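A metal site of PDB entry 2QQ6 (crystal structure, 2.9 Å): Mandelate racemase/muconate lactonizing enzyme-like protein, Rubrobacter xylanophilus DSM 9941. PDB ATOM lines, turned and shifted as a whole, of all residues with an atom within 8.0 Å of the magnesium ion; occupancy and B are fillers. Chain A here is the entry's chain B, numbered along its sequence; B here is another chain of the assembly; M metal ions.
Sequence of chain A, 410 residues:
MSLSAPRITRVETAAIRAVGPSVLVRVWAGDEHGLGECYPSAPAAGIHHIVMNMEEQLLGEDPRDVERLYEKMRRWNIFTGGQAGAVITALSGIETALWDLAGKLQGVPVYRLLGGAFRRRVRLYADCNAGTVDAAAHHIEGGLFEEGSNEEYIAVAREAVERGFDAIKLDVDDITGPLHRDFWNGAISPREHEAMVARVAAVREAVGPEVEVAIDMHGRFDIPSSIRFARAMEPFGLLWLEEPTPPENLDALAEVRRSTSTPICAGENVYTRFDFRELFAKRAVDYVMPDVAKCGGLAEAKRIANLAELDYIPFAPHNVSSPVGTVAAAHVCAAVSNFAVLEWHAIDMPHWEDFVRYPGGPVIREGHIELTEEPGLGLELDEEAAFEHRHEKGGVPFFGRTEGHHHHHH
A ring nitrogen (NE2) of His 318 lies within hydrogen-bond range of the side-chain carboxylate of Glu 268, at 3.2 Å.
The side-chain amino group (NZ) of Lys 169 lies within salt-bridge range of the side-chain carboxylate (OE1) of Glu 242 (2.9 Å).
OE1 of Glu 242 sits at hydrogen-bond distance from NE1 of Trp 240 (3.4 Å).
The backbone carbonyl oxygen (O) of Ile 215 is in hydrogen-bond range of the backbone NH (N) of Glu 242, at 2.7 Å.
The side-chain amino group (NZ) of Lys 169 lies close to the side-chain carboxylate (OD2) of Asp 216, at 3.8 Å.
The side-chain carboxylate (OD1) of Asp 216 is in hydrogen-bond range of the backbone NH (N) of His 218 (2.6 Å).
OE2 of Glu 343 is in salt-bridge range of NZ of Lys 169 (3.8 Å).
The side-chain amino group of Lys 169 lies within hydrogen-bond range of the side-chain hydroxyl of Tyr 125, 3.1 Å away.
NZ of Lys 169 touches the magnesium ion, at 3.4 Å.
NE2 of His 318 touches the magnesium ion, 3.6 Å away.
Within 4 Å of the magnesium ion: Lys 169, Asp 216, Glu 242, Glu 268 and His 318.
The magnesium ion is bound by the side-chain carboxylate of Glu 268 (2.0 Å), the side-chain carboxylate of Glu 242 (2.2 Å) and the side-chain carboxylate of Asp 216 (2.2 Å).
The magnesium ion has three donor atoms within binding distance.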
ATOM      1  N   TYR A  39     -24.707  -0.642   0.050  1.00  0.00           N
ATOM      2  CA  TYR A  39     -23.672  -0.630   1.071  1.00  0.00           C
ATOM      3  C   TYR A  39     -22.343  -0.538   0.312  1.00  0.00           C
ATOM      4  O   TYR A  39     -22.237  -0.977  -0.831  1.00  0.00           O
ATOM      5  CB  TYR A  39     -23.729  -1.924   1.879  1.00  0.00           C
ATOM      6  CG  TYR A  39     -22.493  -2.232   2.694  1.00  0.00           C
ATOM      7  CD1 TYR A  39     -22.366  -1.763   4.006  1.00  0.00           C
ATOM      8  CD2 TYR A  39     -21.437  -2.978   2.148  1.00  0.00           C
ATOM      9  CE1 TYR A  39     -21.209  -2.035   4.739  1.00  0.00           C
ATOM     10  CE2 TYR A  39     -20.284  -3.242   2.877  1.00  0.00           C
ATOM     11  CZ  TYR A  39     -20.181  -2.772   4.170  1.00  0.00           C
ATOM     12  OH  TYR A  39     -19.040  -3.017   4.900  1.00  0.00           O
ATOM     13  N   TYR A 125     -26.514   5.631  17.501  1.00  0.00           N
ATOM     14  CA  TYR A 125     -25.290   5.438  18.279  1.00  0.00           C
ATOM     15  C   TYR A 125     -24.147   5.944  17.394  1.00  0.00           C
ATOM     16  O   TYR A 125     -24.182   5.808  16.158  1.00  0.00           O
ATOM     17  CB  TYR A 125     -25.106   3.974  18.757  1.00  0.00           C
ATOM     18  CG  TYR A 125     -24.609   2.927  17.774  1.00  0.00           C
ATOM     19  CD1 TYR A 125     -23.261   2.844  17.445  1.00  0.00           C
ATOM     20  CD2 TYR A 125     -25.471   1.930  17.286  1.00  0.00           C
ATOM     21  CE1 TYR A 125     -22.766   1.804  16.659  1.00  0.00           C
ATOM     22  CE2 TYR A 125     -24.982   0.881  16.491  1.00  0.00           C
ATOM     23  CZ  TYR A 125     -23.625   0.820  16.189  1.00  0.00           C
ATOM     24  OH  TYR A 125     -23.105  -0.226  15.458  1.00  0.00           O
ATOM     25  N   ASP A 127     -20.290   5.918  16.099  1.00  0.00           N
ATOM     26  CA  ASP A 127     -19.055   5.158  15.978  1.00  0.00           C
ATOM     27  C   ASP A 127     -17.928   6.189  16.152  1.00  0.00           C
ATOM     28  O   ASP A 127     -17.851   7.150  15.401  1.00  0.00           O
ATOM     29  CB  ASP A 127     -18.994   4.491  14.597  1.00  0.00           C
ATOM     30  CG  ASP A 127     -17.849   3.498  14.484  1.00  0.00           C
ATOM     31  OD1 ASP A 127     -16.678   3.935  14.435  1.00  0.00           O
ATOM     32  OD2 ASP A 127     -18.127   2.278  14.442  1.00  0.00           O
ATOM     33  N   ALA A 137     -11.171  -2.389   7.316  1.00  0.00           N
ATOM     34  CA  ALA A 137     -11.332  -2.052   8.728  1.00  0.00           C
ATOM     35  C   ALA A 137     -10.064  -1.984   9.574  1.00  0.00           C
ATOM     36  O   ALA A 137     -10.124  -2.109  10.795  1.00  0.00           O
ATOM     37  CB  ALA A 137     -12.330  -3.013   9.387  1.00  0.00           C
ATOM     38  N   LYS A 169     -19.598   3.866  20.045  1.00  0.00           N
ATOM     39  CA  LYS A 169     -18.975   2.621  19.565  1.00  0.00           C
ATOM     40  C   LYS A 169     -17.468   2.819  19.374  1.00  0.00           C
ATOM     41  O   LYS A 169     -17.030   3.831  18.831  1.00  0.00           O
ATOM     42  CB  LYS A 169     -19.588   2.172  18.236  1.00  0.00           C
ATOM     43  CG  LYS A 169     -19.015   0.860  17.691  1.00  0.00           C
ATOM     44  CD  LYS A 169     -19.612   0.538  16.317  1.00  0.00           C
ATOM     45  CE  LYS A 169     -19.403  -0.917  15.887  1.00  0.00           C
ATOM     46  NZ  LYS A 169     -20.258  -1.295  14.716  1.00  0.00           N
ATOM     47  N   ASP A 171     -13.352   0.835  18.614  1.00  0.00           N
ATOM     48  CA  ASP A 171     -12.529  -0.277  18.130  1.00  0.00           C
ATOM     49  C   ASP A 171     -11.406  -0.585  19.090  1.00  0.00           C
ATOM     50  O   ASP A 171     -11.024   0.266  19.883  1.00  0.00           O
ATOM     51  CB  ASP A 171     -11.877   0.046  16.783  1.00  0.00           C
ATOM     52  CG  ASP A 171     -12.892   0.250  15.684  1.00  0.00           C
ATOM     53  OD1 ASP A 171     -13.997  -0.332  15.775  1.00  0.00           O
ATOM     54  OD2 ASP A 171     -12.565   0.965  14.713  1.00  0.00           O
ATOM     55  N   ILE A 215     -18.145  -2.053  21.922  1.00  0.00           N
ATOM     56  CA  ILE A 215     -16.803  -2.241  21.365  1.00  0.00           C
ATOM     57  C   ILE A 215     -16.704  -3.285  20.243  1.00  0.00           C
ATOM     58  O   ILE A 215     -17.171  -4.410  20.387  1.00  0.00           O
ATOM     59  CB  ILE A 215     -15.851  -2.629  22.506  1.00  0.00           C
ATOM     60  CG1 ILE A 215     -15.702  -1.440  23.457  1.00  0.00           C
ATOM     61  CG2 ILE A 215     -14.519  -3.119  21.953  1.00  0.00           C
ATOM     62  CD1 ILE A 215     -14.887  -1.731  24.686  1.00  0.00           C
ATOM     63  N   ASP A 216     -16.067  -2.900  19.135  1.00  0.00           N
ATOM     64  CA  ASP A 216     -15.918  -3.779  17.974  1.00  0.00           C
ATOM     65  C   ASP A 216     -14.525  -4.383  17.938  1.00  0.00           C
ATOM     66  O   ASP A 216     -13.541  -3.692  18.192  1.00  0.00           O
ATOM     67  CB  ASP A 216     -16.145  -2.971  16.682  1.00  0.00           C
ATOM     68  CG  ASP A 216     -16.451  -3.857  15.469  1.00  0.00           C
ATOM     69  OD1 ASP A 216     -16.021  -5.036  15.429  1.00  0.00           O
ATOM     70  OD2 ASP A 216     -17.089  -3.343  14.537  1.00  0.00           O
ATOM     71  N   MET A 217     -14.453  -5.668  17.612  1.00  0.00           N
ATOM     72  CA  MET A 217     -13.188  -6.383  17.493  1.00  0.00           C
ATOM     73  C   MET A 217     -12.906  -6.759  16.043  1.00  0.00           C
ATOM     74  O   MET A 217     -11.912  -7.405  15.740  1.00  0.00           O
ATOM     75  CB  MET A 217     -13.193  -7.633  18.344  1.00  0.00           C
ATOM     76  CG  MET A 217     -13.282  -7.378  19.831  1.00  0.00           C
ATOM     77  SD  MET A 217     -12.804  -8.978  20.948  1.00  0.00           S
ATOM     78  CE  MET A 217     -14.563  -9.499  21.525  1.00  0.00           C
ATOM     79  N   HIS A 218     -13.800  -6.349  15.155  1.00  0.00           N
ATOM     80  CA  HIS A 218     -13.673  -6.613  13.727  1.00  0.00           C
ATOM     81  C   HIS A 218     -13.318  -8.062  13.404  1.00  0.00           C
ATOM     82  O   HIS A 218     -12.640  -8.332  12.428  1.00  0.00           O
ATOM     83  CB  HIS A 218     -12.666  -5.651  13.104  1.00  0.00           C
ATOM     84  CG  HIS A 218     -13.193  -4.252  12.995  1.00  0.00           C
ATOM     85  ND1 HIS A 218     -12.534  -3.162  13.522  1.00  0.00           N
ATOM     86  CD2 HIS A 218     -14.360  -3.777  12.492  1.00  0.00           C
ATOM     87  CE1 HIS A 218     -13.274  -2.078  13.362  1.00  0.00           C
ATOM     88  NE2 HIS A 218     -14.385  -2.430  12.740  1.00  0.00           N
ATOM     89  N   GLY A 219     -13.812  -8.972  14.257  1.00  0.00           N
ATOM     90  CA  GLY A 219     -13.587 -10.401  14.132  1.00  0.00           C
ATOM     91  C   GLY A 219     -12.242 -10.836  13.594  1.00  0.00           C
ATOM     92  O   GLY A 219     -12.135 -11.276  12.451  1.00  0.00           O
ATOM     93  N   TRP A 240     -22.259  -4.106  24.461  1.00  0.00           N
ATOM     94  CA  TRP A 240     -22.035  -5.407  23.875  1.00  0.00           C
ATOM     95  C   TRP A 240     -20.617  -5.436  23.356  1.00  0.00           C
ATOM     96  O   TRP A 240     -19.925  -4.413  23.318  1.00  0.00           O
ATOM     97  CB  TRP A 240     -23.021  -5.672  22.721  1.00  0.00           C
ATOM     98  CG  TRP A 240     -22.722  -4.985  21.431  1.00  0.00           C
ATOM     99  CD1 TRP A 240     -21.589  -5.107  20.665  1.00  0.00           C
ATOM    100  CD2 TRP A 240     -23.586  -4.093  20.720  1.00  0.00           C
ATOM    101  NE1 TRP A 240     -21.701  -4.361  19.530  1.00  0.00           N
ATOM    102  CE2 TRP A 240     -22.922  -3.727  19.527  1.00  0.00           C
ATOM    103  CE3 TRP A 240     -24.859  -3.581  20.971  1.00  0.00           C
ATOM    104  CZ2 TRP A 240     -23.496  -2.865  18.591  1.00  0.00           C
ATOM    105  CZ3 TRP A 240     -25.434  -2.719  20.035  1.00  0.00           C
ATOM    106  CH2 TRP A 240     -24.742  -2.378  18.860  1.00  0.00           C
ATOM    107  N   GLU A 242     -18.631  -6.657  20.008  1.00  0.00           N
ATOM    108  CA  GLU A 242     -18.806  -7.006  18.592  1.00  0.00           C
ATOM    109  C   GLU A 242     -17.760  -7.916  17.950  1.00  0.00           C
ATOM    110  O   GLU A 242     -16.554  -7.654  18.013  1.00  0.00           O
ATOM    111  CB  GLU A 242     -18.930  -5.706  17.784  1.00  0.00           C
ATOM    112  CG  GLU A 242     -19.544  -5.810  16.377  1.00  0.00           C
ATOM    113  CD  GLU A 242     -19.866  -4.437  15.772  1.00  0.00           C
ATOM    114  OE1 GLU A 242     -20.557  -3.640  16.428  1.00  0.00           O
ATOM    115  OE2 GLU A 242     -19.439  -4.148  14.629  1.00  0.00           O
ATOM    116  N   GLU A 243     -18.229  -8.979  17.313  1.00  0.00           N
ATOM    117  CA  GLU A 243     -17.399  -9.935  16.593  1.00  0.00           C
ATOM    118  C   GLU A 243     -15.997 -10.276  17.103  1.00  0.00           C
ATOM    119  O   GLU A 243     -15.016  -9.819  16.535  1.00  0.00           O
ATOM    120  CB  GLU A 243     -17.247  -9.488  15.130  1.00  0.00           C
ATOM    121  CG  GLU A 243     -18.542  -9.223  14.370  1.00  0.00           C
ATOM    122  CD  GLU A 243     -18.292  -8.710  12.965  1.00  0.00           C
ATOM    123  OE1 GLU A 243     -17.539  -7.720  12.824  1.00  0.00           O
ATOM    124  OE2 GLU A 243     -18.843  -9.283  11.992  1.00  0.00           O
ATOM    125  N   GLU A 268     -23.310  -8.148  10.989  1.00  0.00           N
ATOM    126  CA  GLU A 268     -23.011  -7.336   9.805  1.00  0.00           C
ATOM    127  C   GLU A 268     -22.369  -8.114   8.660  1.00  0.00           C
ATOM    128  O   GLU A 268     -22.299  -7.618   7.532  1.00  0.00           O
ATOM    129  CB  GLU A 268     -22.096  -6.173  10.188  1.00  0.00           C
ATOM    130  CG  GLU A 268     -20.819  -6.574  10.885  1.00  0.00           C
ATOM    131  CD  GLU A 268     -19.875  -5.420  11.036  1.00  0.00           C
ATOM    132  OE1 GLU A 268     -19.427  -4.892   9.995  1.00  0.00           O
ATOM    133  OE2 GLU A 268     -19.568  -5.036  12.189  1.00  0.00           O
ATOM    134  N   ASN A 269     -21.920  -9.327   8.929  1.00  0.00           N
ATOM    135  CA  ASN A 269     -21.295 -10.123   7.886  1.00  0.00           C
ATOM    136  C   ASN A 269     -22.114 -11.341   7.463  1.00  0.00           C
ATOM    137  O   ASN A 269     -21.627 -12.186   6.733  1.00  0.00           O
ATOM    138  CB  ASN A 269     -19.889 -10.539   8.304  1.00  0.00           C
ATOM    139  CG  ASN A 269     -18.920  -9.393   8.276  1.00  0.00           C
ATOM    140  OD1 ASN A 269     -18.839  -8.664   7.295  1.00  0.00           O
ATOM    141  ND2 ASN A 269     -18.159  -9.233   9.349  1.00  0.00           N
ATOM    142  N   MET A 289     -27.290  -7.469  14.419  1.00  0.00           N
ATOM    143  CA  MET A 289     -27.065  -6.240  13.707  1.00  0.00           C
ATOM    144  C   MET A 289     -26.773  -6.387  12.238  1.00  0.00           C
ATOM    145  O   MET A 289     -25.636  -6.205  11.821  1.00  0.00           O
ATOM    146  CB  MET A 289     -25.943  -5.479  14.374  1.00  0.00           C
ATOM    147  CG  MET A 289     -24.685  -6.277  14.508  1.00  0.00           C
ATOM    148  SD  MET A 289     -23.218  -5.186  15.225  1.00  0.00           S
ATOM    149  CE  MET A 289     -22.294  -4.743  13.523  1.00  0.00           C
ATOM    150  N   HIS A 318     -26.458  -2.500  11.555  1.00  0.00           N
ATOM    151  CA  HIS A 318     -25.152  -1.905  11.295  1.00  0.00           C
ATOM    152  C   HIS A 318     -25.425  -0.906  10.160  1.00  0.00           C
ATOM    153  O   HIS A 318     -26.106  -1.239   9.201  1.00  0.00           O
ATOM    154  CB  HIS A 318     -24.175  -3.021  10.869  1.00  0.00           C
ATOM    155  CG  HIS A 318     -22.804  -2.557  10.468  1.00  0.00           C
ATOM    156  ND1 HIS A 318     -22.417  -2.434   9.144  1.00  0.00           N
ATOM    157  CD2 HIS A 318     -21.716  -2.232  11.205  1.00  0.00           C
ATOM    158  CE1 HIS A 318     -21.152  -2.070   9.095  1.00  0.00           C
ATOM    159  NE2 HIS A 318     -20.705  -1.931  10.329  1.00  0.00           N
ATOM    160  N   ASN A 319     -24.922   0.308  10.293  1.00  0.00           N
ATOM    161  CA  ASN A 319     -25.152   1.342   9.290  1.00  0.00           C
ATOM    162  C   ASN A 319     -23.862   2.045   8.917  1.00  0.00           C
ATOM    163  O   ASN A 319     -23.149   2.538   9.780  1.00  0.00           O
ATOM    164  CB  ASN A 319     -26.141   2.375   9.834  1.00  0.00           C
ATOM    165  CG  ASN A 319     -26.601   3.365   8.770  1.00  0.00           C
ATOM    166  OD1 ASN A 319     -25.804   3.919   8.021  1.00  0.00           O
ATOM    167  ND2 ASN A 319     -27.902   3.588   8.725  1.00  0.00           N
ATOM    168  N   GLU A 343     -26.906   2.606  13.935  1.00  0.00           N
ATOM    169  CA  GLU A 343     -25.563   3.148  13.862  1.00  0.00           C
ATOM    170  C   GLU A 343     -25.414   4.326  12.937  1.00  0.00           C
ATOM    171  O   GLU A 343     -26.066   4.421  11.897  1.00  0.00           O
ATOM    172  CB  GLU A 343     -24.570   2.063  13.429  1.00  0.00           C
ATOM    173  CG  GLU A 343     -23.263   2.620  12.894  1.00  0.00           C
ATOM    174  CD  GLU A 343     -22.217   1.551  12.637  1.00  0.00           C
ATOM    175  OE1 GLU A 343     -22.609   0.422  12.282  1.00  0.00           O
ATOM    176  OE2 GLU A 343     -21.015   1.852  12.773  1.00  0.00           O
ATOM    177  N   HIS A 345     -22.088   6.373  11.348  1.00  0.00           N
ATOM    178  CA  HIS A 345     -20.651   6.250  11.194  1.00  0.00           C
ATOM    179  C   HIS A 345     -20.077   7.489  10.493  1.00  0.00           C
ATOM    180  O   HIS A 345     -19.009   7.419   9.887  1.00  0.00           O
ATOM    181  CB  HIS A 345     -20.395   4.973  10.364  1.00  0.00           C
ATOM    182  CG  HIS A 345     -18.986   4.469  10.416  1.00  0.00           C
ATOM    183  ND1 HIS A 345     -17.925   5.136   9.834  1.00  0.00           N
ATOM    184  CD2 HIS A 345     -18.468   3.333  10.953  1.00  0.00           C
ATOM    185  CE1 HIS A 345     -16.819   4.426  10.011  1.00  0.00           C
ATOM    186  NE2 HIS A 345     -17.127   3.331  10.680  1.00  0.00           N
ATOM    187  N   PHE B  79     -15.172  -7.344   4.998  1.00  0.00           N
ATOM    188  CA  PHE B  79     -16.249  -6.366   5.126  1.00  0.00           C
ATOM    189  C   PHE B  79     -16.800  -5.922   3.770  1.00  0.00           C
ATOM    190  O   PHE B  79     -17.534  -4.946   3.687  1.00  0.00           O
ATOM    191  CB  PHE B  79     -15.773  -5.138   5.912  1.00  0.00           C
ATOM    192  CG  PHE B  79     -15.476  -5.432   7.347  1.00  0.00           C
ATOM    193  CD1 PHE B  79     -14.156  -5.564   7.785  1.00  0.00           C
ATOM    194  CD2 PHE B  79     -16.499  -5.587   8.264  1.00  0.00           C
ATOM    195  CE1 PHE B  79     -13.866  -5.877   9.126  1.00  0.00           C
ATOM    196  CE2 PHE B  79     -16.233  -5.899   9.609  1.00  0.00           C
ATOM    197  CZ  PHE B  79     -14.911  -6.035  10.038  1.00  0.00           C
HETATM  198 MG    MG M   1     -18.495  -3.409  12.784  1.00  0.00          MG
